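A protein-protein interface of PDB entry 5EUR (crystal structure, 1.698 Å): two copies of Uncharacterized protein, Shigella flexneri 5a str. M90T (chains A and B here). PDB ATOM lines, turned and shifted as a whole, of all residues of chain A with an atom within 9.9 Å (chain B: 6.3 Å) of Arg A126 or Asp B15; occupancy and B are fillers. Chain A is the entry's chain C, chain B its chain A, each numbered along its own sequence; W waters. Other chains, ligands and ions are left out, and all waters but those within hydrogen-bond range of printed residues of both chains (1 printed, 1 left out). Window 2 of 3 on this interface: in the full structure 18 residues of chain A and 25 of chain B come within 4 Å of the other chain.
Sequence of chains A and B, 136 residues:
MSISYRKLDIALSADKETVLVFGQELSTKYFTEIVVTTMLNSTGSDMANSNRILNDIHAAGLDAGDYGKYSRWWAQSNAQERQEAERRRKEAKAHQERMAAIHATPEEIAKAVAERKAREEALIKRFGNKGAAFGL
The guanidinium group (NH2) of Arg A126 lies within hydrogen-bond range of the side-chain hydroxyl (OG) of Ser B13. The guanidinium group (NE) of Arg A126 lies within salt-bridge range of the side-chain carboxylate (OE2) of Glu B25 (3.0 Å). SD of Met B99 lies close to N of Gly A128. The backbone carbonyl oxygen of Arg A126 sits at hydrogen-bond distance from the backbone NH of Ala B14 (2.8 Å). The side-chain hydroxyl (OG1) of Thr B18 is in hydrogen-bond range of the guanidinium group (NH2) of Arg A126 (2.9 Å). The guanidinium group of Arg A126 is in salt-bridge range of the side-chain carboxylate of Asp B15, at 3.1 Å.
The backbone NH of Ser B13 is in hydrogen-bond range of the backbone carbonyl oxygen of Thr B18, at 2.9 Å. The side-chain hydroxyl (OG1) of Thr B18 lies within hydrogen-bond range of the side-chain carboxylate (OE2) of Glu B25 (2.7 Å). The backbone NH (N) of Glu B17 is in hydrogen-bond range of the side-chain carboxylate (OD1) of Asp B15 (2.9 Å). The backbone carbonyl oxygen (O) of Ser B13 lies within hydrogen-bond range of the side-chain amide nitrogen (NE2) of Gln B96 (3.2 Å). The side-chain hydroxyl (OG) of Ser B13 sits at hydrogen-bond distance from the backbone NH (N) of Lys B16 (3.1 Å). The backbone carbonyl oxygen of Leu B12 is in hydrogen-bond range of the side-chain amide nitrogen of Gln B96, 3.0 Å away.
Glu B25 touches Leu A123. O of Ile A124 touches CE of Met B99, 3.7 Å away. Leu B12 touches Phe A127. Phe A127 touches Ser B13. Phe A127 touches Thr B18. Phe A127 touches Glu B25. Phe A127 touches Met B99.
Arg A126 touches five residues of chain B. Of chain A, only Arg A126 (3.1 Å) comes within 4 Å of Asp B15. Ala B14 touches just one residue of chain A: Arg A126 (2.8 Å). No residue of chain A comes within 4 Å of Glu B17. Of the printed residues of chain A, Met B99 touches Ile A124 (3.7 Å), Phe A127 (3.7 Å) and Gly A128 (3.5 Å). Printed residues of chain A within 4 Å of Glu B25: Leu A123 (3.8 Å), Arg A126 (3.0 Å) and Phe A127 (3.7 Å). Of the printed residues of chain B, Phe A127 touches Leu B12 (3.7 Å), Ser B13 (3.4 Å), Thr B18 (3.5 Å), Glu B25 (3.7 Å) and Met B99 (3.7 Å). Of the printed residues of chain B, Leu A123 touches Glu B25. The nearest residue of chain B that does not touch Arg A126 is Met B99 (4.4 Å). The nearest printed residue of chain A that does not touch Glu B25 is Ala A122 (6.3 Å).
Of the 10 printed residues of chain B, 7 touch a printed residue of chain A. Along chain B the printed residues that touch a printed residue of chain A span positions 12 to 99. Hydrophobic or aromatic side chains of chain A within 4 Å of the printed part of chain B: Leu A123 and Phe A127. Among the printed residues, 13 pairs touch across the chains. Among the printed residues, Asp or Glu carboxylates within 4 Å of a Lys or Arg side-chain nitrogen of the other chain: Arg A126 with Asp B15 (3.1 Å) and Arg A126 with Glu B25 (3.0 Å).
No position is printed for both chains. Of the 13 pairs that touch across the chains among the printed residues, none has its exchanged pair printed and touching as well.
Water W1 bridges the backbone carbonyl oxygen of Leu B12 and the backbone carbonyl oxygen of Phe A127.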
ATOM      1  N   GLU A 120      -4.638  -1.181  -1.156  1.00  0.00           N
ATOM      2  CA  GLU A 120      -3.751  -1.879  -2.017  1.00  0.00           C
ATOM      3  C   GLU A 120      -4.159  -1.542  -3.453  1.00  0.00           C
ATOM      4  O   GLU A 120      -3.507  -1.944  -4.364  1.00  0.00           O
ATOM      5  CB  GLU A 120      -3.864  -3.406  -1.657  1.00  0.00           C
ATOM      6  CG  GLU A 120      -3.193  -3.900  -0.344  1.00  0.00           C
ATOM      7  CD  GLU A 120      -4.116  -4.421   0.784  1.00  0.00           C
ATOM      8  OE1 GLU A 120      -5.249  -3.954   0.905  1.00  0.00           O
ATOM      9  OE2 GLU A 120      -3.706  -5.298   1.576  1.00  0.00           O
ATOM     10  N   GLU A 121      -5.227  -0.785  -3.658  1.00  0.00           N
ATOM     11  CA  GLU A 121      -5.666  -0.476  -5.025  1.00  0.00           C
ATOM     12  C   GLU A 121      -6.667   0.619  -5.196  1.00  0.00           C
ATOM     13  O   GLU A 121      -7.819   0.364  -5.014  1.00  0.00           O
ATOM     14  CB  GLU A 121      -6.252  -1.734  -5.606  1.00  0.00           C
ATOM     15  CG  GLU A 121      -7.094  -2.506  -4.593  1.00  0.00           C
ATOM     16  CD  GLU A 121      -6.505  -3.859  -4.328  1.00  0.00           C
ATOM     17  OE1 GLU A 121      -7.117  -4.887  -4.664  1.00  0.00           O
ATOM     18  OE2 GLU A 121      -5.421  -3.896  -3.795  1.00  0.00           O
ATOM     19  N   ALA A 122      -6.279   1.833  -5.581  1.00  0.00           N
ATOM     20  CA  ALA A 122      -4.921   2.256  -5.829  1.00  0.00           C
ATOM     21  C   ALA A 122      -4.158   1.819  -7.096  1.00  0.00           C
ATOM     22  O   ALA A 122      -3.594   2.622  -7.796  1.00  0.00           O
ATOM     23  CB  ALA A 122      -4.023   1.828  -4.716  1.00  0.00           C
ATOM     24  N   LEU A 123      -4.174   0.541  -7.349  1.00  0.00           N
ATOM     25  CA  LEU A 123      -3.723   0.015  -8.606  1.00  0.00           C
ATOM     26  C   LEU A 123      -4.904   0.075  -9.553  1.00  0.00           C
ATOM     27  O   LEU A 123      -4.741   0.128 -10.716  1.00  0.00           O
ATOM     28  CB  LEU A 123      -3.257  -1.398  -8.438  1.00  0.00           C
ATOM     29  CG  LEU A 123      -1.991  -1.514  -7.613  1.00  0.00           C
ATOM     30  CD1 LEU A 123      -1.710  -2.959  -7.333  1.00  0.00           C
ATOM     31  CD2 LEU A 123      -0.799  -0.813  -8.213  1.00  0.00           C
ATOM     32  N   ILE A 124      -6.113   0.079  -9.016  1.00  0.00           N
ATOM     33  CA  ILE A 124      -7.296   0.130  -9.838  1.00  0.00           C
ATOM     34  C   ILE A 124      -7.331   1.453 -10.591  1.00  0.00           C
ATOM     35  O   ILE A 124      -7.557   1.487 -11.761  1.00  0.00           O
ATOM     36  CB  ILE A 124      -8.560  -0.178  -9.003  1.00  0.00           C
ATOM     37  CG1 ILE A 124      -8.752  -1.668  -8.941  1.00  0.00           C
ATOM     38  CG2 ILE A 124      -9.799   0.471  -9.589  1.00  0.00           C
ATOM     39  CD1 ILE A 124     -10.072  -2.085  -8.371  1.00  0.00           C
ATOM     40  N   LYS A 125      -7.087   2.536  -9.909  1.00  0.00           N
ATOM     41  CA  LYS A 125      -7.070   3.809 -10.574  1.00  0.00           C
ATOM     42  C   LYS A 125      -6.031   3.830 -11.687  1.00  0.00           C
ATOM     43  O   LYS A 125      -6.166   4.567 -12.648  1.00  0.00           O
ATOM     44  CB  LYS A 125      -6.734   4.913  -9.592  1.00  0.00           C
ATOM     45  CG  LYS A 125      -7.926   5.557  -8.913  1.00  0.00           C
ATOM     46  CD  LYS A 125      -8.882   6.219  -9.897  1.00  0.00           C
ATOM     47  CE  LYS A 125     -10.316   6.055  -9.478  1.00  0.00           C
ATOM     48  NZ  LYS A 125     -10.687   4.651  -9.171  1.00  0.00           N
ATOM     49  N   ARG A 126      -4.971   3.041 -11.559  1.00  0.00           N
ATOM     50  CA  ARG A 126      -3.889   3.057 -12.557  1.00  0.00           C
ATOM     51  C   ARG A 126      -4.032   2.033 -13.658  1.00  0.00           C
ATOM     52  O   ARG A 126      -3.775   2.296 -14.786  1.00  0.00           O
ATOM     53  CB  ARG A 126      -2.500   2.927 -11.889  1.00  0.00           C
ATOM     54  CG  ARG A 126      -1.998   4.186 -11.200  1.00  0.00           C
ATOM     55  CD  ARG A 126      -0.544   4.089 -10.757  1.00  0.00           C
ATOM     56  NE  ARG A 126       0.363   4.106 -11.872  1.00  0.00           N
ATOM     57  CZ  ARG A 126       0.599   5.158 -12.640  1.00  0.00           C
ATOM     58  NH1 ARG A 126      -0.019   6.290 -12.384  1.00  0.00           N
ATOM     59  NH2 ARG A 126       1.443   5.081 -13.648  1.00  0.00           N
ATOM     60  N   PHE A 127      -4.452   0.856 -13.275  1.00  0.00           N
ATOM     61  CA  PHE A 127      -4.543  -0.250 -14.177  1.00  0.00           C
ATOM     62  C   PHE A 127      -5.944  -0.830 -14.414  1.00  0.00           C
ATOM     63  O   PHE A 127      -6.095  -1.679 -15.234  1.00  0.00           O
ATOM     64  CB  PHE A 127      -3.657  -1.390 -13.623  1.00  0.00           C
ATOM     65  CG  PHE A 127      -2.221  -1.015 -13.427  1.00  0.00           C
ATOM     66  CD1 PHE A 127      -1.350  -0.988 -14.470  1.00  0.00           C
ATOM     67  CD2 PHE A 127      -1.767  -0.677 -12.207  1.00  0.00           C
ATOM     68  CE1 PHE A 127      -0.079  -0.588 -14.296  1.00  0.00           C
ATOM     69  CE2 PHE A 127      -0.465  -0.311 -12.018  1.00  0.00           C
ATOM     70  CZ  PHE A 127       0.382  -0.268 -13.081  1.00  0.00           C
ATOM     71  N   GLY A 128      -6.936  -0.377 -13.665  1.00  0.00           N
ATOM     72  CA  GLY A 128      -8.255  -0.974 -13.732  1.00  0.00           C
ATOM     73  C   GLY A 128      -8.340  -2.402 -13.243  1.00  0.00           C
ATOM     74  O   GLY A 128      -9.453  -2.891 -13.003  1.00  0.00           O
ATOM     75  N   ASN A 129      -7.209  -3.085 -13.077  1.00  0.00           N
ATOM     76  CA  ASN A 129      -7.163  -4.478 -12.653  1.00  0.00           C
ATOM     77  C   ASN A 129      -5.739  -4.857 -12.247  1.00  0.00           C
ATOM     78  O   ASN A 129      -5.449  -5.088 -11.071  1.00  0.00           O
ATOM     79  CB  ASN A 129      -7.661  -5.392 -13.766  1.00  0.00           C
ATOM     80  N   LEU B  12      -0.578  -2.573 -18.505  1.00  0.00           N
ATOM     81  CA  LEU B  12      -0.040  -1.246 -18.756  1.00  0.00           C
ATOM     82  C   LEU B  12      -0.939  -0.208 -18.093  1.00  0.00           C
ATOM     83  O   LEU B  12      -2.168  -0.292 -18.176  1.00  0.00           O
ATOM     84  CB  LEU B  12       0.057  -1.013 -20.268  1.00  0.00           C
ATOM     85  CG  LEU B  12       0.698   0.238 -20.862  1.00  0.00           C
ATOM     86  CD1 LEU B  12       2.119   0.401 -20.366  1.00  0.00           C
ATOM     87  CD2 LEU B  12       0.707   0.132 -22.379  1.00  0.00           C
ATOM     88  N   SER B  13      -0.324   0.754 -17.415  1.00  0.00           N
ATOM     89  CA  SER B  13      -1.068   1.790 -16.714  1.00  0.00           C
ATOM     90  C   SER B  13      -1.804   2.687 -17.708  1.00  0.00           C
ATOM     91  O   SER B  13      -1.450   2.778 -18.884  1.00  0.00           O
ATOM     92  CB  SER B  13      -0.129   2.638 -15.850  1.00  0.00           C
ATOM     93  OG  SER B  13       0.703   3.487 -16.637  1.00  0.00           O
ATOM     94  N   ALA B  14      -2.831   3.381 -17.207  1.00  0.00           N
ATOM     95  CA  ALA B  14      -3.622   4.245 -18.079  1.00  0.00           C
ATOM     96  C   ALA B  14      -2.762   5.336 -18.709  1.00  0.00           C
ATOM     97  O   ALA B  14      -2.897   5.629 -19.902  1.00  0.00           O
ATOM     98  CB  ALA B  14      -4.782   4.853 -17.293  1.00  0.00           C
ATOM     99  N   ASP B  15      -1.856   5.933 -17.937  1.00  0.00           N
ATOM    100  CA  ASP B  15      -0.971   6.938 -18.514  1.00  0.00           C
ATOM    101  C   ASP B  15       0.232   6.331 -19.220  1.00  0.00           C
ATOM    102  O   ASP B  15       1.074   7.080 -19.726  1.00  0.00           O
ATOM    103  CB  ASP B  15      -0.522   7.946 -17.445  1.00  0.00           C
ATOM    104  CG  ASP B  15       0.307   7.323 -16.333  1.00  0.00           C
ATOM    105  OD1 ASP B  15       0.807   6.187 -16.483  1.00  0.00           O
ATOM    106  OD2 ASP B  15       0.462   7.989 -15.290  1.00  0.00           O
ATOM    107  N   LYS B  16       0.324   4.998 -19.262  1.00  0.00           N
ATOM    108  CA  LYS B  16       1.347   4.198 -19.932  1.00  0.00           C
ATOM    109  C   LYS B  16       2.719   4.316 -19.289  1.00  0.00           C
ATOM    110  O   LYS B  16       3.680   3.742 -19.818  1.00  0.00           O
ATOM    111  CB  LYS B  16       1.494   4.529 -21.428  1.00  0.00           C
ATOM    112  CG  LYS B  16       0.198   4.813 -22.190  1.00  0.00           C
ATOM    113  CD  LYS B  16      -0.474   3.528 -22.648  1.00  0.00           C
ATOM    114  CE  LYS B  16      -1.576   3.794 -23.679  1.00  0.00           C
ATOM    115  NZ  LYS B  16      -2.640   4.710 -23.176  1.00  0.00           N
ATOM    116  N   GLU B  17       2.857   5.029 -18.174  1.00  0.00           N
ATOM    117  CA  GLU B  17       4.193   5.255 -17.636  1.00  0.00           C
ATOM    118  C   GLU B  17       4.694   4.098 -16.782  1.00  0.00           C
ATOM    119  O   GLU B  17       5.908   3.986 -16.580  1.00  0.00           O
ATOM    120  CB  GLU B  17       4.241   6.554 -16.830  1.00  0.00           C
ATOM    121  CG  GLU B  17       4.173   7.794 -17.714  1.00  0.00           C
ATOM    122  CD  GLU B  17       4.317   9.088 -16.935  1.00  0.00           C
ATOM    123  OE1 GLU B  17       4.478   9.034 -15.696  1.00  0.00           O
ATOM    124  OE2 GLU B  17       4.278  10.163 -17.570  1.00  0.00           O
ATOM    125  N   THR B  18       3.806   3.241 -16.282  1.00  0.00           N
ATOM    126  CA  THR B  18       4.234   2.070 -15.523  1.00  0.00           C
ATOM    127  C   THR B  18       3.520   0.819 -16.021  1.00  0.00           C
ATOM    128  O   THR B  18       2.499   0.877 -16.712  1.00  0.00           O
ATOM    129  CB  THR B  18       3.992   2.228 -14.005  1.00  0.00           C
ATOM    130  OG1 THR B  18       2.590   2.373 -13.743  1.00  0.00           O
ATOM    131  CG2 THR B  18       4.768   3.415 -13.432  1.00  0.00           C
ATOM    132  N   GLU B  25       4.997  -3.172  -9.589  1.00  0.00           N
ATOM    133  CA  GLU B  25       4.916  -1.997 -10.440  1.00  0.00           C
ATOM    134  C   GLU B  25       6.323  -1.549 -10.814  1.00  0.00           C
ATOM    135  O   GLU B  25       7.204  -1.434  -9.950  1.00  0.00           O
ATOM    136  CB  GLU B  25       4.141  -0.866  -9.755  1.00  0.00           C
ATOM    137  CG  GLU B  25       3.876   0.292 -10.703  1.00  0.00           C
ATOM    138  CD  GLU B  25       2.793   1.245 -10.218  1.00  0.00           C
ATOM    139  OE1 GLU B  25       2.361   1.132  -9.049  1.00  0.00           O
ATOM    140  OE2 GLU B  25       2.378   2.110 -11.021  1.00  0.00           O
ATOM    141  N   GLN B  96      -7.932   0.171 -22.335  1.00  0.00           N
ATOM    142  CA  GLN B  96      -7.331   1.500 -22.249  1.00  0.00           C
ATOM    143  C   GLN B  96      -8.309   2.581 -22.691  1.00  0.00           C
ATOM    144  O   GLN B  96      -8.325   3.685 -22.130  1.00  0.00           O
ATOM    145  CB  GLN B  96      -6.063   1.558 -23.101  1.00  0.00           C
ATOM    146  CG  GLN B  96      -4.884   0.823 -22.493  1.00  0.00           C
ATOM    147  CD  GLN B  96      -4.188   1.648 -21.426  1.00  0.00           C
ATOM    148  OE1 GLN B  96      -4.287   2.879 -21.412  1.00  0.00           O
ATOM    149  NE2 GLN B  96      -3.488   0.975 -20.520  1.00  0.00           N
ATOM    150  N   MET B  99     -10.837   3.098 -20.012  1.00  0.00           N
ATOM    151  CA  MET B  99     -10.203   3.798 -18.899  1.00  0.00           C
ATOM    152  C   MET B  99     -10.016   5.275 -19.206  1.00  0.00           C
ATOM    153  O   MET B  99     -10.098   6.110 -18.298  1.00  0.00           O
ATOM    154  CB  MET B  99      -8.857   3.166 -18.562  1.00  0.00           C
ATOM    155  CG  MET B  99      -8.960   1.796 -17.936  1.00  0.00           C
ATOM    156  SD  MET B  99      -7.626   1.544 -16.761  1.00  0.00           S
ATOM    157  CE  MET B  99      -8.334   2.322 -15.312  1.00  0.00           C
HETATM  158  O   HOH W   1      -4.147  -2.076 -17.561  1.00  0.00           O
